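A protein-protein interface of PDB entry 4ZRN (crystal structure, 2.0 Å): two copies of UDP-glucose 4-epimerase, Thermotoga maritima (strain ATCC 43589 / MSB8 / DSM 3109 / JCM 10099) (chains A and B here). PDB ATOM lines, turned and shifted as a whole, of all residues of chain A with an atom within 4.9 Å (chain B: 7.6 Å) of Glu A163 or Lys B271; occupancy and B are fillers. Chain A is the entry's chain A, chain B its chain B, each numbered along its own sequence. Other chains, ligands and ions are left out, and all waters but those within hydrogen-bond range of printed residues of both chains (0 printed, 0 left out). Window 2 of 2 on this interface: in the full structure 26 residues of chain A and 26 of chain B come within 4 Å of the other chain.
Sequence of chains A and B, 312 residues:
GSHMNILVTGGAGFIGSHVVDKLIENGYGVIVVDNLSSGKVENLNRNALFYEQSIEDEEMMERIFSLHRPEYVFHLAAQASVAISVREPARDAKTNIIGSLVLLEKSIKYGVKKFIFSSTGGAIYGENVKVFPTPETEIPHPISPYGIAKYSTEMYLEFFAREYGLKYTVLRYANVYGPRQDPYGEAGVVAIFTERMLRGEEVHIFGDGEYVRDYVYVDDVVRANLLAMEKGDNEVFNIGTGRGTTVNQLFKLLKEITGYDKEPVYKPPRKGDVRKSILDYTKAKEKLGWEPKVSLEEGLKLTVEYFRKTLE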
ATOM      1  N   PHE A 159      -0.261 -40.201  10.003  1.00  0.00           N
ATOM      2  CA  PHE A 159      -0.751 -38.835  10.127  1.00  0.00           C
ATOM      3  C   PHE A 159      -1.020 -38.453  11.581  1.00  0.00           C
ATOM      4  O   PHE A 159      -0.624 -37.369  12.039  1.00  0.00           O
ATOM      5  CB  PHE A 159      -2.013 -38.601   9.303  1.00  0.00           C
ATOM      6  CG  PHE A 159      -2.799 -37.409   9.773  1.00  0.00           C
ATOM      7  CD1 PHE A 159      -2.343 -36.126   9.510  1.00  0.00           C
ATOM      8  CD2 PHE A 159      -3.964 -37.573  10.517  1.00  0.00           C
ATOM      9  CE1 PHE A 159      -3.048 -35.017   9.968  1.00  0.00           C
ATOM     10  CE2 PHE A 159      -4.678 -36.469  10.977  1.00  0.00           C
ATOM     11  CZ  PHE A 159      -4.218 -35.192  10.698  1.00  0.00           C
ATOM     12  N   PHE A 160      -1.710 -39.325  12.309  1.00  0.00           N
ATOM     13  CA  PHE A 160      -2.037 -39.016  13.702  1.00  0.00           C
ATOM     14  C   PHE A 160      -0.773 -38.920  14.553  1.00  0.00           C
ATOM     15  O   PHE A 160      -0.685 -38.079  15.448  1.00  0.00           O
ATOM     16  CB  PHE A 160      -3.053 -40.015  14.294  1.00  0.00           C
ATOM     17  CG  PHE A 160      -4.479 -39.698  13.941  1.00  0.00           C
ATOM     18  CD1 PHE A 160      -5.229 -38.856  14.746  1.00  0.00           C
ATOM     19  CD2 PHE A 160      -5.068 -40.225  12.788  1.00  0.00           C
ATOM     20  CE1 PHE A 160      -6.545 -38.550  14.421  1.00  0.00           C
ATOM     21  CE2 PHE A 160      -6.385 -39.917  12.447  1.00  0.00           C
ATOM     22  CZ  PHE A 160      -7.126 -39.077  13.269  1.00  0.00           C
ATOM     23  N   ALA A 161       0.213 -39.764  14.263  1.00  0.00           N
ATOM     24  CA  ALA A 161       1.494 -39.677  14.970  1.00  0.00           C
ATOM     25  C   ALA A 161       2.200 -38.339  14.702  1.00  0.00           C
ATOM     26  O   ALA A 161       2.688 -37.685  15.634  1.00  0.00           O
ATOM     27  CB  ALA A 161       2.393 -40.846  14.597  1.00  0.00           C
ATOM     28  N   ARG A 162       2.255 -37.938  13.435  1.00  0.00           N
ATOM     29  CA  ARG A 162       2.924 -36.694  13.056  1.00  0.00           C
ATOM     30  C   ARG A 162       2.221 -35.469  13.615  1.00  0.00           C
ATOM     31  O   ARG A 162       2.863 -34.582  14.173  1.00  0.00           O
ATOM     32  CB  ARG A 162       3.024 -36.568  11.532  1.00  0.00           C
ATOM     33  CG  ARG A 162       3.917 -37.611  10.860  1.00  0.00           C
ATOM     34  CD  ARG A 162       3.914 -37.448   9.336  1.00  0.00           C
ATOM     35  NE  ARG A 162       4.268 -36.085   8.942  1.00  0.00           N
ATOM     36  CZ  ARG A 162       5.395 -35.743   8.321  1.00  0.00           C
ATOM     37  NH1 ARG A 162       6.289 -36.669   7.991  1.00  0.00           N
ATOM     38  NH2 ARG A 162       5.621 -34.469   8.018  1.00  0.00           N
ATOM     39  N   GLU A 163       0.901 -35.422  13.455  1.00  0.00           N
ATOM     40  CA  GLU A 163       0.122 -34.246  13.821  1.00  0.00           C
ATOM     41  C   GLU A 163      -0.074 -34.092  15.328  1.00  0.00           C
ATOM     42  O   GLU A 163      -0.004 -32.979  15.843  1.00  0.00           O
ATOM     43  CB  GLU A 163      -1.236 -34.261  13.106  1.00  0.00           C
ATOM     44  CG  GLU A 163      -2.097 -33.024  13.342  1.00  0.00           C
ATOM     45  CD  GLU A 163      -1.596 -31.790  12.599  1.00  0.00           C
ATOM     46  OE1 GLU A 163      -2.087 -30.686  12.903  1.00  0.00           O
ATOM     47  OE2 GLU A 163      -0.735 -31.917  11.705  1.00  0.00           O
ATOM     48  N   TYR A 164      -0.314 -35.196  16.037  1.00  0.00           N
ATOM     49  CA  TYR A 164      -0.713 -35.112  17.441  1.00  0.00           C
ATOM     50  C   TYR A 164       0.225 -35.820  18.413  1.00  0.00           C
ATOM     51  O   TYR A 164       0.083 -35.673  19.624  1.00  0.00           O
ATOM     52  CB  TYR A 164      -2.129 -35.658  17.629  1.00  0.00           C
ATOM     53  CG  TYR A 164      -3.194 -34.942  16.831  1.00  0.00           C
ATOM     54  CD1 TYR A 164      -3.647 -33.683  17.210  1.00  0.00           C
ATOM     55  CD2 TYR A 164      -3.757 -35.531  15.700  1.00  0.00           C
ATOM     56  CE1 TYR A 164      -4.629 -33.031  16.487  1.00  0.00           C
ATOM     57  CE2 TYR A 164      -4.736 -34.879  14.967  1.00  0.00           C
ATOM     58  CZ  TYR A 164      -5.169 -33.630  15.370  1.00  0.00           C
ATOM     59  OH  TYR A 164      -6.149 -32.980  14.646  1.00  0.00           O
ATOM     60  N   GLY A 165       1.170 -36.598  17.896  1.00  0.00           N
ATOM     61  CA  GLY A 165       2.117 -37.280  18.759  1.00  0.00           C
ATOM     62  C   GLY A 165       1.617 -38.604  19.297  1.00  0.00           C
ATOM     63  O   GLY A 165       2.190 -39.158  20.234  1.00  0.00           O
ATOM     64  N   VAL B  82      -7.269 -28.880   2.416  1.00  0.00           N
ATOM     65  CA  VAL B  82      -6.341 -29.673   3.242  1.00  0.00           C
ATOM     66  C   VAL B  82      -6.440 -29.380   4.749  1.00  0.00           C
ATOM     67  O   VAL B  82      -6.259 -30.290   5.564  1.00  0.00           O
ATOM     68  CB  VAL B  82      -4.855 -29.607   2.743  1.00  0.00           C
ATOM     69  CG1 VAL B  82      -3.992 -30.640   3.464  1.00  0.00           C
ATOM     70  CG2 VAL B  82      -4.763 -29.830   1.226  1.00  0.00           C
ATOM     71  N   VAL B  86      -7.852 -32.114   8.395  1.00  0.00           N
ATOM     72  CA  VAL B  86      -6.985 -32.385   9.544  1.00  0.00           C
ATOM     73  C   VAL B  86      -7.765 -32.499  10.844  1.00  0.00           C
ATOM     74  O   VAL B  86      -7.462 -33.343  11.688  1.00  0.00           O
ATOM     75  CB  VAL B  86      -5.890 -31.299   9.668  1.00  0.00           C
ATOM     76  CG1 VAL B  86      -5.107 -31.424  10.991  1.00  0.00           C
ATOM     77  CG2 VAL B  86      -4.960 -31.372   8.485  1.00  0.00           C
ATOM     78  N   ARG B  87      -8.793 -31.673  11.004  1.00  0.00           N
ATOM     79  CA  ARG B  87      -9.517 -31.638  12.271  1.00  0.00           C
ATOM     80  C   ARG B  87     -10.651 -32.661  12.357  1.00  0.00           C
ATOM     81  O   ARG B  87     -10.967 -33.168  13.442  1.00  0.00           O
ATOM     82  CB  ARG B  87     -10.027 -30.220  12.565  1.00  0.00           C
ATOM     83  CG  ARG B  87      -8.952 -29.237  13.073  1.00  0.00           C
ATOM     84  CD  ARG B  87      -7.951 -28.817  11.975  1.00  0.00           C
ATOM     85  NE  ARG B  87      -7.774 -27.363  11.896  1.00  0.00           N
ATOM     86  CZ  ARG B  87      -6.918 -26.741  11.083  1.00  0.00           C
ATOM     87  NH1 ARG B  87      -6.137 -27.439  10.258  1.00  0.00           N
ATOM     88  NH2 ARG B  87      -6.841 -25.412  11.094  1.00  0.00           N
ATOM     89  N   ILE B 143       0.790 -37.560   3.492  1.00  0.00           N
ATOM     90  CA  ILE B 143       0.843 -37.491   4.941  1.00  0.00           C
ATOM     91  C   ILE B 143      -0.299 -36.658   5.515  1.00  0.00           C
ATOM     92  O   ILE B 143      -0.418 -36.553   6.727  1.00  0.00           O
ATOM     93  CB  ILE B 143       2.169 -36.883   5.410  1.00  0.00           C
ATOM     94  CG1 ILE B 143       2.324 -35.484   4.815  1.00  0.00           C
ATOM     95  CG2 ILE B 143       3.335 -37.785   5.027  1.00  0.00           C
ATOM     96  CD1 ILE B 143       3.671 -34.872   5.064  1.00  0.00           C
ATOM     97  N   PRO B 145      -4.612 -35.997   5.557  1.00  0.00           N
ATOM     98  CA  PRO B 145      -5.798 -36.831   5.336  1.00  0.00           C
ATOM     99  C   PRO B 145      -6.375 -36.660   3.931  1.00  0.00           C
ATOM    100  O   PRO B 145      -6.876 -37.631   3.337  1.00  0.00           O
ATOM    101  CB  PRO B 145      -6.773 -36.340   6.419  1.00  0.00           C
ATOM    102  CG  PRO B 145      -5.840 -35.882   7.551  1.00  0.00           C
ATOM    103  CD  PRO B 145      -4.734 -35.178   6.781  1.00  0.00           C
ATOM    104  N   PHE B 206       2.637 -16.058   3.673  1.00  0.00           N
ATOM    105  CA  PHE B 206       3.021 -16.942   4.771  1.00  0.00           C
ATOM    106  C   PHE B 206       4.511 -17.303   4.700  1.00  0.00           C
ATOM    107  O   PHE B 206       5.022 -17.660   3.630  1.00  0.00           O
ATOM    108  CB  PHE B 206       2.166 -18.217   4.734  1.00  0.00           C
ATOM    109  CG  PHE B 206       0.683 -17.958   4.799  1.00  0.00           C
ATOM    110  CD1 PHE B 206       0.181 -16.860   5.493  1.00  0.00           C
ATOM    111  CD2 PHE B 206      -0.210 -18.814   4.170  1.00  0.00           C
ATOM    112  CE1 PHE B 206      -1.200 -16.620   5.554  1.00  0.00           C
ATOM    113  CE2 PHE B 206      -1.583 -18.587   4.221  1.00  0.00           C
ATOM    114  CZ  PHE B 206      -2.081 -17.485   4.915  1.00  0.00           C
ATOM    115  N   TYR B 211       7.811 -20.572  -1.186  1.00  0.00           N
ATOM    116  CA  TYR B 211       7.115 -21.798  -1.568  1.00  0.00           C
ATOM    117  C   TYR B 211       6.816 -21.808  -3.064  1.00  0.00           C
ATOM    118  O   TYR B 211       6.261 -20.852  -3.602  1.00  0.00           O
ATOM    119  CB  TYR B 211       5.817 -21.964  -0.766  1.00  0.00           C
ATOM    120  CG  TYR B 211       6.078 -21.957   0.722  1.00  0.00           C
ATOM    121  CD1 TYR B 211       6.414 -23.126   1.401  1.00  0.00           C
ATOM    122  CD2 TYR B 211       6.027 -20.773   1.442  1.00  0.00           C
ATOM    123  CE1 TYR B 211       6.676 -23.110   2.768  1.00  0.00           C
ATOM    124  CE2 TYR B 211       6.283 -20.745   2.801  1.00  0.00           C
ATOM    125  CZ  TYR B 211       6.607 -21.912   3.457  1.00  0.00           C
ATOM    126  OH  TYR B 211       6.863 -21.870   4.812  1.00  0.00           O
ATOM    127  N   PRO B 268       3.211 -15.734   9.917  1.00  0.00           N
ATOM    128  CA  PRO B 268       4.026 -16.929  10.174  1.00  0.00           C
ATOM    129  C   PRO B 268       3.762 -18.025   9.137  1.00  0.00           C
ATOM    130  O   PRO B 268       2.688 -18.030   8.525  1.00  0.00           O
ATOM    131  CB  PRO B 268       3.555 -17.376  11.566  1.00  0.00           C
ATOM    132  CG  PRO B 268       3.100 -16.092  12.226  1.00  0.00           C
ATOM    133  CD  PRO B 268       2.445 -15.317  11.110  1.00  0.00           C
ATOM    134  N   PRO B 269       4.739 -18.925   8.928  1.00  0.00           N
ATOM    135  CA  PRO B 269       4.578 -20.023   7.966  1.00  0.00           C
ATOM    136  C   PRO B 269       3.376 -20.870   8.337  1.00  0.00           C
ATOM    137  O   PRO B 269       3.076 -21.009   9.522  1.00  0.00           O
ATOM    138  CB  PRO B 269       5.873 -20.835   8.117  1.00  0.00           C
ATOM    139  CG  PRO B 269       6.492 -20.368   9.429  1.00  0.00           C
ATOM    140  CD  PRO B 269       6.054 -18.945   9.592  1.00  0.00           C
ATOM    141  N   ARG B 270       2.685 -21.402   7.337  1.00  0.00           N
ATOM    142  CA  ARG B 270       1.488 -22.199   7.569  1.00  0.00           C
ATOM    143  C   ARG B 270       1.922 -23.653   7.721  1.00  0.00           C
ATOM    144  O   ARG B 270       2.629 -24.194   6.865  1.00  0.00           O
ATOM    145  CB  ARG B 270       0.526 -22.026   6.392  1.00  0.00           C
ATOM    146  CG  ARG B 270      -0.873 -22.572   6.588  1.00  0.00           C
ATOM    147  CD  ARG B 270      -1.736 -22.244   5.368  1.00  0.00           C
ATOM    148  NE  ARG B 270      -1.243 -22.893   4.156  1.00  0.00           N
ATOM    149  CZ  ARG B 270      -1.842 -22.831   2.970  1.00  0.00           C
ATOM    150  NH1 ARG B 270      -2.968 -22.139   2.827  1.00  0.00           N
ATOM    151  NH2 ARG B 270      -1.323 -23.472   1.927  1.00  0.00           N
ATOM    152  N   LYS B 271       1.524 -24.278   8.823  1.00  0.00           N
ATOM    153  CA  LYS B 271       1.990 -25.625   9.137  1.00  0.00           C
ATOM    154  C   LYS B 271       1.634 -26.616   8.021  1.00  0.00           C
ATOM    155  O   LYS B 271       0.521 -26.584   7.490  1.00  0.00           O
ATOM    156  CB  LYS B 271       1.400 -26.092  10.469  1.00  0.00           C
ATOM    157  CG  LYS B 271       1.936 -27.437  10.927  1.00  0.00           C
ATOM    158  CD  LYS B 271       1.001 -28.082  11.945  1.00  0.00           C
ATOM    159  CE  LYS B 271       1.623 -29.350  12.503  1.00  0.00           C
ATOM    160  NZ  LYS B 271       2.274 -30.146  11.416  1.00  0.00           N
ATOM    161  N   GLY B 272       2.588 -27.455   7.636  1.00  0.00           N
ATOM    162  CA  GLY B 272       2.330 -28.477   6.633  1.00  0.00           C
ATOM    163  C   GLY B 272       2.572 -28.120   5.167  1.00  0.00           C
ATOM    164  O   GLY B 272       2.448 -28.988   4.296  1.00  0.00           O
ATOM    165  N   ASP B 273       2.902 -26.862   4.873  1.00  0.00           N
ATOM    166  CA  ASP B 273       3.153 -26.455   3.483  1.00  0.00           C
ATOM    167  C   ASP B 273       4.404 -27.139   2.929  1.00  0.00           C
ATOM    168  O   ASP B 273       5.497 -26.917   3.442  1.00  0.00           O
ATOM    169  CB  ASP B 273       3.368 -24.935   3.384  1.00  0.00           C
ATOM    170  CG  ASP B 273       2.072 -24.131   3.413  1.00  0.00           C
ATOM    171  OD1 ASP B 273       0.965 -24.718   3.364  1.00  0.00           O
ATOM    172  OD2 ASP B 273       2.175 -22.883   3.473  1.00  0.00           O
ATOM    173  N   VAL B 274       4.276 -27.955   1.884  1.00  0.00           N
ATOM    174  CA  VAL B 274       5.497 -28.472   1.267  1.00  0.00           C
ATOM    175  C   VAL B 274       6.225 -27.318   0.612  1.00  0.00           C
ATOM    176  O   VAL B 274       5.606 -26.328   0.196  1.00  0.00           O
ATOM    177  CB  VAL B 274       5.272 -29.596   0.243  1.00  0.00           C
ATOM    178  CG1 VAL B 274       4.777 -30.859   0.936  1.00  0.00           C
ATOM    179  CG2 VAL B 274       4.334 -29.142  -0.883  1.00  0.00           C
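Printed residues of chain A that touch a printed residue of chain B: Phe A159, Arg A162, Glu A163 and Tyr A164.
Hydrophobic or aromatic side chains of chain A within 4 Å of the printed part of chain B: Phe A159 and Tyr A164.
Of the 14 printed residues of chain B, 4 touch a printed residue of chain A.
Hydrophobic or aromatic side chains of chain B that line the printed part of chain A: Val B86, Ile B143 and Pro B145.
Among the printed residues, 7 pairs touch across the chains.
Among the printed residues, Asp or Glu carboxylates within 4 Å of a Lys or Arg side-chain nitrogen of the other chain: Glu A163 with Lys B271 (3.5 Å).
No position is printed for both chains.
Among the printed residues, merely in contact across the chains: Phe A159 with Ile B143 (3.4 Å), Arg A162 with Ile B143 (3.6 Å), Phe A159 with Pro B145 (3.6 Å), Glu A163 with Val B86 (3.6 Å) and Phe A159 with Val B86 (3.9 Å).
The side-chain hydroxyl (OH) of Tyr A164 sits at hydrogen-bond distance from the backbone carbonyl oxygen (O) of Val B86 (3.3 Å).
OE2 of Glu A163 lies within salt-bridge range of NZ of Lys B271, 3.5 Å away.
Printed residues of chain B within 4 Å of Phe A159: Val B86 (3.9 Å), Ile B143 (3.4 Å) and Pro B145 (3.6 Å).
Of chain B, only Val B86 and Lys B271 come within 4 Å of Glu A163.
Of the printed residues of chain B, Tyr A164 touches Val B86 (3.3 Å).
Of the printed residues of chain A, Val B86 touches Phe A159, Glu A163 and Tyr A164.
Of the printed residues of chain A, Ile B143 touches Phe A159 (3.4 Å) and Arg A162 (3.6 Å).
Printed residues of chain A within 4 Å of Pro B145: Phe A159 (3.6 Å).
Of chain A, only Glu A163 (3.5 Å) comes within 4 Å of Lys B271.
The nearest printed residue of chain A that does not touch Lys B271 is Arg A162 (5.3 Å).
The nearest printed residue of chain B that does not touch Arg A162 is Lys B271 (5.3 Å).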
